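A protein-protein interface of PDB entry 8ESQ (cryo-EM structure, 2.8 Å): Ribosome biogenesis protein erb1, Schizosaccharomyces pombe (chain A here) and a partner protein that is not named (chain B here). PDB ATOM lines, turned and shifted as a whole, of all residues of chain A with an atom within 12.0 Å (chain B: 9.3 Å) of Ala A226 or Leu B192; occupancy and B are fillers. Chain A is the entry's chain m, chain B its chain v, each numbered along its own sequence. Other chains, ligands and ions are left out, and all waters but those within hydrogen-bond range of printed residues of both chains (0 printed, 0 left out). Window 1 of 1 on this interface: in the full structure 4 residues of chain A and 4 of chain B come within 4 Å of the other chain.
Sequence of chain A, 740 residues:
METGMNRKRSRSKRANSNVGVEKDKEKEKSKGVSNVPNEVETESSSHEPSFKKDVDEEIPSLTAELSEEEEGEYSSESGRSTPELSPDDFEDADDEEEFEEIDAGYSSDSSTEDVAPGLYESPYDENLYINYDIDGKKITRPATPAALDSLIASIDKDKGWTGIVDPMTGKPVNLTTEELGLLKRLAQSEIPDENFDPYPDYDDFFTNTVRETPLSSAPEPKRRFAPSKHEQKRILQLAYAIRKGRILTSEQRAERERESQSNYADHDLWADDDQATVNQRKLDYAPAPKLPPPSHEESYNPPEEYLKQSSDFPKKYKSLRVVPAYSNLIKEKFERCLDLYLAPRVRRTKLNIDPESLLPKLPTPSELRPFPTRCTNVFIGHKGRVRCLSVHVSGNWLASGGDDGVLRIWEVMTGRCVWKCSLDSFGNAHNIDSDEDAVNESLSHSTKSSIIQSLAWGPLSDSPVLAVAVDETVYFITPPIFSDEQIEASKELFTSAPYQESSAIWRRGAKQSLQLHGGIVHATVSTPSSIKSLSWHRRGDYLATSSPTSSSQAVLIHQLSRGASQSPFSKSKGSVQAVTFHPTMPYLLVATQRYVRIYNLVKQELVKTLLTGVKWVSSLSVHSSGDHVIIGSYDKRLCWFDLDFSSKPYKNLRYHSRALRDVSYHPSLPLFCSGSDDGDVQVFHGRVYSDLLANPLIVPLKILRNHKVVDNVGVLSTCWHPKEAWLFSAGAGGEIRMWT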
ATOM      1  N   PRO A 219     -20.945  35.296 -41.727  1.00  0.00           N
ATOM      2  CA  PRO A 219     -19.824  34.811 -40.921  1.00  0.00           C
ATOM      3  C   PRO A 219     -20.090  33.424 -40.362  1.00  0.00           C
ATOM      4  O   PRO A 219     -21.231  33.043 -40.087  1.00  0.00           O
ATOM      5  CB  PRO A 219     -19.723  35.851 -39.804  1.00  0.00           C
ATOM      6  CG  PRO A 219     -21.125  36.318 -39.634  1.00  0.00           C
ATOM      7  CD  PRO A 219     -21.745  36.302 -41.006  1.00  0.00           C
ATOM      8  N   GLU A 220     -19.014  32.674 -40.187  1.00  0.00           N
ATOM      9  CA  GLU A 220     -19.112  31.309 -39.685  1.00  0.00           C
ATOM     10  C   GLU A 220     -19.385  31.319 -38.186  1.00  0.00           C
ATOM     11  O   GLU A 220     -18.644  31.955 -37.433  1.00  0.00           O
ATOM     12  CB  GLU A 220     -17.825  30.548 -39.978  1.00  0.00           C
ATOM     13  CG  GLU A 220     -18.012  29.058 -40.178  1.00  0.00           C
ATOM     14  CD  GLU A 220     -18.544  28.716 -41.556  1.00  0.00           C
ATOM     15  OE1 GLU A 220     -18.380  29.538 -42.481  1.00  0.00           O
ATOM     16  OE2 GLU A 220     -19.121  27.621 -41.715  1.00  0.00           O
ATOM     17  N   PRO A 221     -20.432  30.643 -37.720  1.00  0.00           N
ATOM     18  CA  PRO A 221     -20.692  30.581 -36.278  1.00  0.00           C
ATOM     19  C   PRO A 221     -19.672  29.697 -35.572  1.00  0.00           C
ATOM     20  O   PRO A 221     -18.901  28.964 -36.191  1.00  0.00           O
ATOM     21  CB  PRO A 221     -22.102  29.990 -36.197  1.00  0.00           C
ATOM     22  CG  PRO A 221     -22.276  29.255 -37.469  1.00  0.00           C
ATOM     23  CD  PRO A 221     -21.499  30.000 -38.503  1.00  0.00           C
ATOM     24  N   LYS A 222     -19.671  29.782 -34.243  1.00  0.00           N
ATOM     25  CA  LYS A 222     -18.732  29.013 -33.439  1.00  0.00           C
ATOM     26  C   LYS A 222     -19.219  27.609 -33.116  1.00  0.00           C
ATOM     27  O   LYS A 222     -18.433  26.809 -32.602  1.00  0.00           O
ATOM     28  CB  LYS A 222     -18.425  29.736 -32.126  1.00  0.00           C
ATOM     29  CG  LYS A 222     -17.918  31.142 -32.294  1.00  0.00           C
ATOM     30  CD  LYS A 222     -17.888  31.864 -30.969  1.00  0.00           C
ATOM     31  CE  LYS A 222     -16.614  31.566 -30.216  1.00  0.00           C
ATOM     32  NZ  LYS A 222     -16.563  32.284 -28.917  1.00  0.00           N
ATOM     33  N   ARG A 223     -20.486  27.289 -33.387  1.00  0.00           N
ATOM     34  CA  ARG A 223     -20.963  25.934 -33.135  1.00  0.00           C
ATOM     35  C   ARG A 223     -20.181  24.922 -33.953  1.00  0.00           C
ATOM     36  O   ARG A 223     -19.938  23.797 -33.504  1.00  0.00           O
ATOM     37  CB  ARG A 223     -22.448  25.812 -33.464  1.00  0.00           C
ATOM     38  CG  ARG A 223     -23.241  27.073 -33.340  1.00  0.00           C
ATOM     39  CD  ARG A 223     -24.678  26.804 -33.732  1.00  0.00           C
ATOM     40  NE  ARG A 223     -24.863  26.755 -35.176  1.00  0.00           N
ATOM     41  CZ  ARG A 223     -25.271  27.780 -35.908  1.00  0.00           C
ATOM     42  NH1 ARG A 223     -25.510  28.963 -35.368  1.00  0.00           N
ATOM     43  NH2 ARG A 223     -25.439  27.618 -37.217  1.00  0.00           N
ATOM     44  N   ARG A 224     -19.794  25.302 -35.168  1.00  0.00           N
ATOM     45  CA  ARG A 224     -19.125  24.390 -36.077  1.00  0.00           C
ATOM     46  C   ARG A 224     -17.700  24.082 -35.655  1.00  0.00           C
ATOM     47  O   ARG A 224     -17.079  23.191 -36.243  1.00  0.00           O
ATOM     48  CB  ARG A 224     -19.166  24.974 -37.486  1.00  0.00           C
ATOM     49  CG  ARG A 224     -20.589  25.167 -37.981  1.00  0.00           C
ATOM     50  CD  ARG A 224     -20.645  25.744 -39.373  1.00  0.00           C
ATOM     51  NE  ARG A 224     -21.978  26.242 -39.685  1.00  0.00           N
ATOM     52  CZ  ARG A 224     -22.279  26.933 -40.772  1.00  0.00           C
ATOM     53  NH1 ARG A 224     -21.367  27.216 -41.684  1.00  0.00           N
ATOM     54  NH2 ARG A 224     -23.527  27.352 -40.950  1.00  0.00           N
ATOM     55  N   PHE A 225     -17.173  24.788 -34.656  1.00  0.00           N
ATOM     56  CA  PHE A 225     -15.831  24.546 -34.152  1.00  0.00           C
ATOM     57  C   PHE A 225     -15.801  24.033 -32.722  1.00  0.00           C
ATOM     58  O   PHE A 225     -14.753  23.562 -32.276  1.00  0.00           O
ATOM     59  CB  PHE A 225     -14.989  25.826 -34.241  1.00  0.00           C
ATOM     60  CG  PHE A 225     -14.918  26.406 -35.622  1.00  0.00           C
ATOM     61  CD1 PHE A 225     -15.919  27.230 -36.099  1.00  0.00           C
ATOM     62  CD2 PHE A 225     -13.850  26.119 -36.446  1.00  0.00           C
ATOM     63  CE1 PHE A 225     -15.850  27.759 -37.366  1.00  0.00           C
ATOM     64  CE2 PHE A 225     -13.778  26.645 -37.710  1.00  0.00           C
ATOM     65  CZ  PHE A 225     -14.781  27.465 -38.171  1.00  0.00           C
ATOM     66  N   ALA A 226     -16.873  24.102 -32.029  1.00  0.00           N
ATOM     67  CA  ALA A 226     -17.010  23.613 -30.673  1.00  0.00           C
ATOM     68  C   ALA A 226     -17.856  22.347 -30.646  1.00  0.00           C
ATOM     69  O   ALA A 226     -18.703  22.147 -31.519  1.00  0.00           O
ATOM     70  CB  ALA A 226     -17.658  24.677 -29.783  1.00  0.00           C
ATOM     71  N   PRO A 227     -17.643  21.465 -29.664  1.00  0.00           N
ATOM     72  CA  PRO A 227     -18.476  20.259 -29.557  1.00  0.00           C
ATOM     73  C   PRO A 227     -19.961  20.575 -29.538  1.00  0.00           C
ATOM     74  O   PRO A 227     -20.368  21.683 -29.177  1.00  0.00           O
ATOM     75  CB  PRO A 227     -18.019  19.624 -28.236  1.00  0.00           C
ATOM     76  CG  PRO A 227     -17.044  20.590 -27.624  1.00  0.00           C
ATOM     77  CD  PRO A 227     -16.513  21.425 -28.727  1.00  0.00           C
ATOM     78  N   SER A 228     -20.779  19.603 -29.922  1.00  0.00           N
ATOM     79  CA  SER A 228     -22.190  19.851 -30.168  1.00  0.00           C
ATOM     80  C   SER A 228     -22.924  20.156 -28.870  1.00  0.00           C
ATOM     81  O   SER A 228     -22.682  19.520 -27.842  1.00  0.00           O
ATOM     82  CB  SER A 228     -22.819  18.650 -30.863  1.00  0.00           C
ATOM     83  OG  SER A 228     -22.909  17.556 -29.987  1.00  0.00           O
ATOM     84  N   LYS A 229     -23.814  21.149 -28.923  1.00  0.00           N
ATOM     85  CA  LYS A 229     -24.599  21.523 -27.754  1.00  0.00           C
ATOM     86  C   LYS A 229     -25.866  20.693 -27.622  1.00  0.00           C
ATOM     87  O   LYS A 229     -26.369  20.520 -26.507  1.00  0.00           O
ATOM     88  CB  LYS A 229     -24.951  23.006 -27.810  1.00  0.00           C
ATOM     89  CG  LYS A 229     -23.756  23.918 -27.768  1.00  0.00           C
ATOM     90  CD  LYS A 229     -24.187  25.363 -27.667  1.00  0.00           C
ATOM     91  CE  LYS A 229     -24.998  25.611 -26.410  1.00  0.00           C
ATOM     92  NZ  LYS A 229     -25.224  27.061 -26.180  1.00  0.00           N
ATOM     93  N   HIS A 230     -26.407  20.192 -28.733  1.00  0.00           N
ATOM     94  CA  HIS A 230     -27.555  19.297 -28.652  1.00  0.00           C
ATOM     95  C   HIS A 230     -27.199  18.033 -27.884  1.00  0.00           C
ATOM     96  O   HIS A 230     -27.981  17.548 -27.060  1.00  0.00           O
ATOM     97  CB  HIS A 230     -28.058  18.928 -30.047  1.00  0.00           C
ATOM     98  CG  HIS A 230     -28.037  20.055 -31.028  1.00  0.00           C
ATOM     99  ND1 HIS A 230     -28.916  21.116 -30.963  1.00  0.00           N
ATOM    100  CD2 HIS A 230     -27.265  20.273 -32.118  1.00  0.00           C
ATOM    101  CE1 HIS A 230     -28.676  21.945 -31.963  1.00  0.00           C
ATOM    102  NE2 HIS A 230     -27.676  21.458 -32.675  1.00  0.00           N
ATOM    103  N   GLU A 231     -26.023  17.473 -28.162  1.00  0.00           N
ATOM    104  CA  GLU A 231     -25.614  16.250 -27.487  1.00  0.00           C
ATOM    105  C   GLU A 231     -25.240  16.511 -26.039  1.00  0.00           C
ATOM    106  O   GLU A 231     -25.520  15.680 -25.171  1.00  0.00           O
ATOM    107  CB  GLU A 231     -24.450  15.610 -28.233  1.00  0.00           C
ATOM    108  CG  GLU A 231     -24.844  15.050 -29.578  1.00  0.00           C
ATOM    109  CD  GLU A 231     -23.784  14.158 -30.165  1.00  0.00           C
ATOM    110  OE1 GLU A 231     -22.706  14.038 -29.554  1.00  0.00           O
ATOM    111  OE2 GLU A 231     -24.024  13.580 -31.243  1.00  0.00           O
ATOM    112  N   GLN A 232     -24.610  17.652 -25.758  1.00  0.00           N
ATOM    113  CA  GLN A 232     -24.308  17.995 -24.374  1.00  0.00           C
ATOM    114  C   GLN A 232     -25.581  18.170 -23.564  1.00  0.00           C
ATOM    115  O   GLN A 232     -25.638  17.781 -22.395  1.00  0.00           O
ATOM    116  CB  GLN A 232     -23.451  19.255 -24.312  1.00  0.00           C
ATOM    117  CG  GLN A 232     -22.948  19.574 -22.920  1.00  0.00           C
ATOM    118  CD  GLN A 232     -22.333  18.375 -22.241  1.00  0.00           C
ATOM    119  OE1 GLN A 232     -22.719  18.011 -21.134  1.00  0.00           O
ATOM    120  NE2 GLN A 232     -21.365  17.754 -22.898  1.00  0.00           N
ATOM    121  N   LYS A 233     -26.613  18.762 -24.165  1.00  0.00           N
ATOM    122  CA  LYS A 233     -27.912  18.801 -23.505  1.00  0.00           C
ATOM    123  C   LYS A 233     -28.464  17.396 -23.306  1.00  0.00           C
ATOM    124  O   LYS A 233     -28.963  17.064 -22.228  1.00  0.00           O
ATOM    125  CB  LYS A 233     -28.888  19.655 -24.312  1.00  0.00           C
ATOM    126  CG  LYS A 233     -30.339  19.430 -23.949  1.00  0.00           C
ATOM    127  CD  LYS A 233     -31.273  20.204 -24.855  1.00  0.00           C
ATOM    128  CE  LYS A 233     -31.842  21.417 -24.148  1.00  0.00           C
ATOM    129  NZ  LYS A 233     -32.995  22.003 -24.879  1.00  0.00           N
ATOM    130  N   ILE A 235     -26.712  14.637 -23.140  1.00  0.00           N
ATOM    131  CA  ILE A 235     -25.857  13.947 -22.175  1.00  0.00           C
ATOM    132  C   ILE A 235     -26.262  14.297 -20.749  1.00  0.00           C
ATOM    133  O   ILE A 235     -26.317  13.427 -19.873  1.00  0.00           O
ATOM    134  CB  ILE A 235     -24.377  14.278 -22.447  1.00  0.00           C
ATOM    135  CG1 ILE A 235     -23.855  13.452 -23.623  1.00  0.00           C
ATOM    136  CG2 ILE A 235     -23.527  14.026 -21.215  1.00  0.00           C
ATOM    137  CD1 ILE A 235     -22.563  13.957 -24.194  1.00  0.00           C
ATOM    138  N   TYR B 166     -13.775  24.313 -15.103  1.00  0.00           N
ATOM    139  CA  TYR B 166     -13.565  24.918 -16.413  1.00  0.00           C
ATOM    140  C   TYR B 166     -12.785  26.221 -16.298  1.00  0.00           C
ATOM    141  O   TYR B 166     -11.771  26.418 -16.977  1.00  0.00           O
ATOM    142  CB  TYR B 166     -14.915  25.153 -17.093  1.00  0.00           C
ATOM    143  CG  TYR B 166     -14.831  25.404 -18.581  1.00  0.00           C
ATOM    144  CD1 TYR B 166     -14.510  26.659 -19.075  1.00  0.00           C
ATOM    145  CD2 TYR B 166     -15.083  24.388 -19.488  1.00  0.00           C
ATOM    146  CE1 TYR B 166     -14.434  26.891 -20.429  1.00  0.00           C
ATOM    147  CE2 TYR B 166     -15.012  24.614 -20.844  1.00  0.00           C
ATOM    148  CZ  TYR B 166     -14.689  25.866 -21.307  1.00  0.00           C
ATOM    149  OH  TYR B 166     -14.617  26.096 -22.658  1.00  0.00           O
ATOM    150  N   LEU B 170      -8.562  27.389 -16.891  1.00  0.00           N
ATOM    151  CA  LEU B 170      -8.226  28.524 -17.744  1.00  0.00           C
ATOM    152  C   LEU B 170      -7.443  29.581 -16.976  1.00  0.00           C
ATOM    153  O   LEU B 170      -6.526  30.205 -17.521  1.00  0.00           O
ATOM    154  CB  LEU B 170      -9.500  29.123 -18.339  1.00  0.00           C
ATOM    155  CG  LEU B 170      -9.973  28.546 -19.674  1.00  0.00           C
ATOM    156  CD1 LEU B 170     -11.336  29.097 -20.036  1.00  0.00           C
ATOM    157  CD2 LEU B 170      -8.972  28.868 -20.762  1.00  0.00           C
ATOM    158  N   MET B 182      -7.633  33.907 -22.980  1.00  0.00           N
ATOM    159  CA  MET B 182      -8.313  32.690 -22.552  1.00  0.00           C
ATOM    160  C   MET B 182      -9.349  32.256 -23.579  1.00  0.00           C
ATOM    161  O   MET B 182      -9.513  31.059 -23.838  1.00  0.00           O
ATOM    162  CB  MET B 182      -8.959  32.903 -21.184  1.00  0.00           C
ATOM    163  CG  MET B 182      -8.031  32.602 -20.028  1.00  0.00           C
ATOM    164  SD  MET B 182      -8.085  33.843 -18.724  1.00  0.00           S
ATOM    165  CE  MET B 182      -9.603  33.387 -17.900  1.00  0.00           C
ATOM    166  N   ALA B 183     -10.059  33.218 -24.170  1.00  0.00           N
ATOM    167  CA  ALA B 183     -11.030  32.901 -25.213  1.00  0.00           C
ATOM    168  C   ALA B 183     -10.356  32.243 -26.410  1.00  0.00           C
ATOM    169  O   ALA B 183     -10.817  31.210 -26.908  1.00  0.00           O
ATOM    170  CB  ALA B 183     -11.762  34.170 -25.640  1.00  0.00           C
ATOM    171  N   LYS B 184      -9.256  32.829 -26.883  1.00  0.00           N
ATOM    172  CA  LYS B 184      -8.568  32.303 -28.053  1.00  0.00           C
ATOM    173  C   LYS B 184      -7.864  30.983 -27.774  1.00  0.00           C
ATOM    174  O   LYS B 184      -7.407  30.330 -28.717  1.00  0.00           O
ATOM    175  CB  LYS B 184      -7.562  33.327 -28.572  1.00  0.00           C
ATOM    176  CG  LYS B 184      -8.194  34.597 -29.108  1.00  0.00           C
ATOM    177  CD  LYS B 184      -7.134  35.545 -29.637  1.00  0.00           C
ATOM    178  CE  LYS B 184      -7.714  36.916 -29.946  1.00  0.00           C
ATOM    179  NZ  LYS B 184      -8.609  36.894 -31.133  1.00  0.00           N
ATOM    180  N   ASP B 185      -7.749  30.584 -26.510  1.00  0.00           N
ATOM    181  CA  ASP B 185      -7.154  29.296 -26.182  1.00  0.00           C
ATOM    182  C   ASP B 185      -8.105  28.195 -26.626  1.00  0.00           C
ATOM    183  O   ASP B 185      -9.223  28.085 -26.117  1.00  0.00           O
ATOM    184  CB  ASP B 185      -6.878  29.220 -24.677  1.00  0.00           C
ATOM    185  CG  ASP B 185      -6.392  27.849 -24.211  1.00  0.00           C
ATOM    186  OD1 ASP B 185      -6.427  26.861 -24.972  1.00  0.00           O
ATOM    187  OD2 ASP B 185      -5.959  27.762 -23.046  1.00  0.00           O
ATOM    188  N   VAL B 186      -7.655  27.369 -27.568  1.00  0.00           N
ATOM    189  CA  VAL B 186      -8.555  26.412 -28.200  1.00  0.00           C
ATOM    190  C   VAL B 186      -8.626  25.112 -27.409  1.00  0.00           C
ATOM    191  O   VAL B 186      -9.669  24.449 -27.382  1.00  0.00           O
ATOM    192  CB  VAL B 186      -8.124  26.174 -29.658  1.00  0.00           C
ATOM    193  CG1 VAL B 186      -8.149  27.482 -30.421  1.00  0.00           C
ATOM    194  CG2 VAL B 186      -6.735  25.567 -29.716  1.00  0.00           C
ATOM    195  N   LYS B 187      -7.531  24.724 -26.754  1.00  0.00           N
ATOM    196  CA  LYS B 187      -7.518  23.457 -26.032  1.00  0.00           C
ATOM    197  C   LYS B 187      -8.321  23.546 -24.741  1.00  0.00           C
ATOM    198  O   LYS B 187      -9.198  22.712 -24.486  1.00  0.00           O
ATOM    199  CB  LYS B 187      -6.078  23.035 -25.744  1.00  0.00           C
ATOM    200  CG  LYS B 187      -5.378  22.381 -26.922  1.00  0.00           C
ATOM    201  CD  LYS B 187      -5.887  20.969 -27.149  1.00  0.00           C
ATOM    202  CE  LYS B 187      -5.145  20.292 -28.286  1.00  0.00           C
ATOM    203  NZ  LYS B 187      -5.712  18.953 -28.601  1.00  0.00           N
ATOM    204  N   LEU B 188      -8.040  24.553 -23.914  1.00  0.00           N
ATOM    205  CA  LEU B 188      -8.703  24.643 -22.617  1.00  0.00           C
ATOM    206  C   LEU B 188     -10.128  25.169 -22.742  1.00  0.00           C
ATOM    207  O   LEU B 188     -11.029  24.691 -22.047  1.00  0.00           O
ATOM    208  CB  LEU B 188      -7.892  25.526 -21.672  1.00  0.00           C
ATOM    209  CG  LEU B 188      -6.501  24.996 -21.323  1.00  0.00           C
ATOM    210  CD1 LEU B 188      -5.798  25.928 -20.353  1.00  0.00           C
ATOM    211  CD2 LEU B 188      -6.583  23.589 -20.771  1.00  0.00           C
ATOM    212  N   ASN B 189     -10.350  26.149 -23.615  1.00  0.00           N
ATOM    213  CA  ASN B 189     -11.693  26.672 -23.861  1.00  0.00           C
ATOM    214  C   ASN B 189     -12.333  25.900 -25.015  1.00  0.00           C
ATOM    215  O   ASN B 189     -12.477  26.385 -26.138  1.00  0.00           O
ATOM    216  CB  ASN B 189     -11.638  28.167 -24.144  1.00  0.00           C
ATOM    217  CG  ASN B 189     -12.994  28.820 -24.074  1.00  0.00           C
ATOM    218  OD1 ASN B 189     -13.935  28.266 -23.512  1.00  0.00           O
ATOM    219  ND2 ASN B 189     -13.105  30.009 -24.650  1.00  0.00           N
ATOM    220  N   SER B 190     -12.725  24.660 -24.711  1.00  0.00           N
ATOM    221  CA  SER B 190     -13.296  23.800 -25.742  1.00  0.00           C
ATOM    222  C   SER B 190     -14.711  24.223 -26.104  1.00  0.00           C
ATOM    223  O   SER B 190     -15.142  24.029 -27.245  1.00  0.00           O
ATOM    224  CB  SER B 190     -13.277  22.343 -25.283  1.00  0.00           C
ATOM    225  OG  SER B 190     -14.070  22.164 -24.126  1.00  0.00           O
ATOM    226  N   LYS B 191     -15.446  24.795 -25.155  1.00  0.00           N
ATOM    227  CA  LYS B 191     -16.773  25.315 -25.441  1.00  0.00           C
ATOM    228  C   LYS B 191     -16.737  26.587 -26.271  1.00  0.00           C
ATOM    229  O   LYS B 191     -17.798  27.054 -26.699  1.00  0.00           O
ATOM    230  CB  LYS B 191     -17.521  25.571 -24.138  1.00  0.00           C
ATOM    231  CG  LYS B 191     -17.793  24.320 -23.341  1.00  0.00           C
ATOM    232  CD  LYS B 191     -18.917  23.530 -23.961  1.00  0.00           C
ATOM    233  CE  LYS B 191     -19.441  22.489 -23.002  1.00  0.00           C
ATOM    234  NZ  LYS B 191     -20.223  23.125 -21.920  1.00  0.00           N
ATOM    235  N   LEU B 192     -15.551  27.154 -26.498  1.00  0.00           N
ATOM    236  CA  LEU B 192     -15.383  28.394 -27.253  1.00  0.00           C
ATOM    237  C   LEU B 192     -16.140  29.547 -26.603  1.00  0.00           C
ATOM    238  O   LEU B 192     -16.798  30.340 -27.278  1.00  0.00           O
ATOM    239  CB  LEU B 192     -15.807  28.224 -28.711  1.00  0.00           C
ATOM    240  CG  LEU B 192     -14.845  27.494 -29.643  1.00  0.00           C
ATOM    241  CD1 LEU B 192     -15.149  27.860 -31.079  1.00  0.00           C
ATOM    242  CD2 LEU B 192     -13.412  27.830 -29.294  1.00  0.00           C
ATOM    243  N   PHE B 193     -16.054  29.638 -25.281  1.00  0.00           N
ATOM    244  CA  PHE B 193     -16.596  30.791 -24.582  1.00  0.00           C
ATOM    245  C   PHE B 193     -15.798  32.039 -24.934  1.00  0.00           C
ATOM    246  O   PHE B 193     -14.581  31.991 -25.125  1.00  0.00           O
ATOM    247  CB  PHE B 193     -16.565  30.569 -23.075  1.00  0.00           C
ATOM    248  CG  PHE B 193     -17.512  29.518 -22.594  1.00  0.00           C
ATOM    249  CD1 PHE B 193     -18.621  29.172 -23.342  1.00  0.00           C
ATOM    250  CD2 PHE B 193     -17.292  28.871 -21.393  1.00  0.00           C
ATOM    251  CE1 PHE B 193     -19.493  28.206 -22.898  1.00  0.00           C
ATOM    252  CE2 PHE B 193     -18.159  27.905 -20.947  1.00  0.00           C
ATOM    253  CZ  PHE B 193     -19.261  27.571 -21.699  1.00  0.00           C
ATOM    254  N   ASN B 194     -16.495  33.167 -25.023  1.00  0.00           N
ATOM    255  CA  ASN B 194     -15.840  34.430 -25.306  1.00  0.00           C
ATOM    256  C   ASN B 194     -15.371  35.072 -24.003  1.00  0.00           C
ATOM    257  O   ASN B 194     -15.660  34.591 -22.905  1.00  0.00           O
ATOM    258  CB  ASN B 194     -16.772  35.353 -26.084  1.00  0.00           C
ATOM    259  CG  ASN B 194     -18.115  35.506 -25.423  1.00  0.00           C
ATOM    260  OD1 ASN B 194     -18.674  34.543 -24.906  1.00  0.00           O
ATOM    261  ND2 ASN B 194     -18.645  36.721 -25.435  1.00  0.00           N
ATOM    262  N   GLY B 195     -14.632  36.175 -24.126  1.00  0.00           N
ATOM    263  CA  GLY B 195     -14.067  36.813 -22.949  1.00  0.00           C
ATOM    264  C   GLY B 195     -15.120  37.294 -21.970  1.00  0.00           C
ATOM    265  O   GLY B 195     -14.910  37.264 -20.756  1.00  0.00           O
ATOM    266  N   SER B 196     -16.262  37.753 -22.483  1.00  0.00           N
ATOM    267  CA  SER B 196     -17.324  38.226 -21.603  1.00  0.00           C
ATOM    268  C   SER B 196     -17.907  37.090 -20.771  1.00  0.00           C
ATOM    269  O   SER B 196     -18.233  37.283 -19.595  1.00  0.00           O
ATOM    270  CB  SER B 196     -18.419  38.913 -22.416  1.00  0.00           C
ATOM    271  OG  SER B 196     -19.241  37.960 -23.061  1.00  0.00           O
ATOM    272  N   LYS B 197     -18.061  35.904 -21.363  1.00  0.00           N
ATOM    273  CA  LYS B 197     -18.581  34.773 -20.601  1.00  0.00           C
ATOM    274  C   LYS B 197     -17.523  34.202 -19.668  1.00  0.00           C
ATOM    275  O   LYS B 197     -17.848  33.672 -18.600  1.00  0.00           O
ATOM    276  CB  LYS B 197     -19.110  33.689 -21.537  1.00  0.00           C
ATOM    277  CG  LYS B 197     -20.116  32.763 -20.870  1.00  0.00           C
ATOM    278  CD  LYS B 197     -20.502  31.611 -21.775  1.00  0.00           C
ATOM    279  CE  LYS B 197     -21.448  30.647 -21.083  1.00  0.00           C
ATOM    280  NZ  LYS B 197     -22.859  31.101 -21.178  1.00  0.00           N
ATOM    281  N   LEU B 198     -16.251  34.288 -20.057  1.00  0.00           N
ATOM    282  CA  LEU B 198     -15.179  33.845 -19.172  1.00  0.00           C
ATOM    283  C   LEU B 198     -15.014  34.793 -17.996  1.00  0.00           C
ATOM    284  O   LEU B 198     -14.540  34.389 -16.928  1.00  0.00           O
ATOM    285  CB  LEU B 198     -13.873  33.713 -19.947  1.00  0.00           C
ATOM    286  CG  LEU B 198     -13.892  32.640 -21.031  1.00  0.00           C
ATOM    287  CD1 LEU B 198     -12.538  32.523 -21.687  1.00  0.00           C
ATOM    288  CD2 LEU B 198     -14.302  31.314 -20.433  1.00  0.00           C
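The side-chain amino group (NZ) of Lys A222 lies within hydrogen-bond range of the backbone carbonyl oxygen (O) of Leu B192.
The side-chain hydroxyl (OH) of Tyr B166 is in hydrogen-bond range of the backbone NH (N) of Ser B190. OH of Tyr B166 is in hydrogen-bond range of N of Lys B191, at 2.9 Å. OG of Ser B196 sits at hydrogen-bond distance from ND2 of Asn B194.
Among the printed residues, merely in contact across the chains: Pro A227 with Ser B190, Ala A226 with Ser B190, Phe A225 with Leu B192, Ala A226 with Lys B191, Ala A226 with Leu B192 and Lys A222 with Asn B194.
Printed residues of chain B within 4 Å of Ala A226: Ser B190, Lys B191 and Leu B192. Printed residues of chain B within 4 Å of Pro A227: Ser B190. Ala B183 touches none of the printed residues of chain A. No residue of chain A comes within 4 Å of Asn B189. Ser B190 touches two residues of chain A. Lys B191 touches just one residue of chain A: Ala A226 (3.9 Å). No residue of chain A comes within 4 Å of Phe B193. Printed residues of chain A within 4 Å of Asn B194: Lys A222. Of the printed residues of chain B, Lys A222 touches Leu B192 (2.6 Å) and Asn B194 (3.99 Å). Of the printed residues of chain B, Phe A225 touches Leu B192. Glu A231 touches none of the printed residues of chain B. Leu B198 touches none of the printed residues of chain A. The nearest printed residue of chain B that does not touch Phe A225 is Ser B190 (5.1 Å).
Of the 16 printed residues of chain A, 4 touch a printed residue of chain B. Of the 19 printed residues of chain B, 4 touch a printed residue of chain A. Printed residues of chain B that touch a printed residue of chain A: Ser B190, Lys B191, Leu B192 and Asn B194. Hydrophobic or aromatic side chains of chain B within 4 Å of the printed part of chain A: Leu B192.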
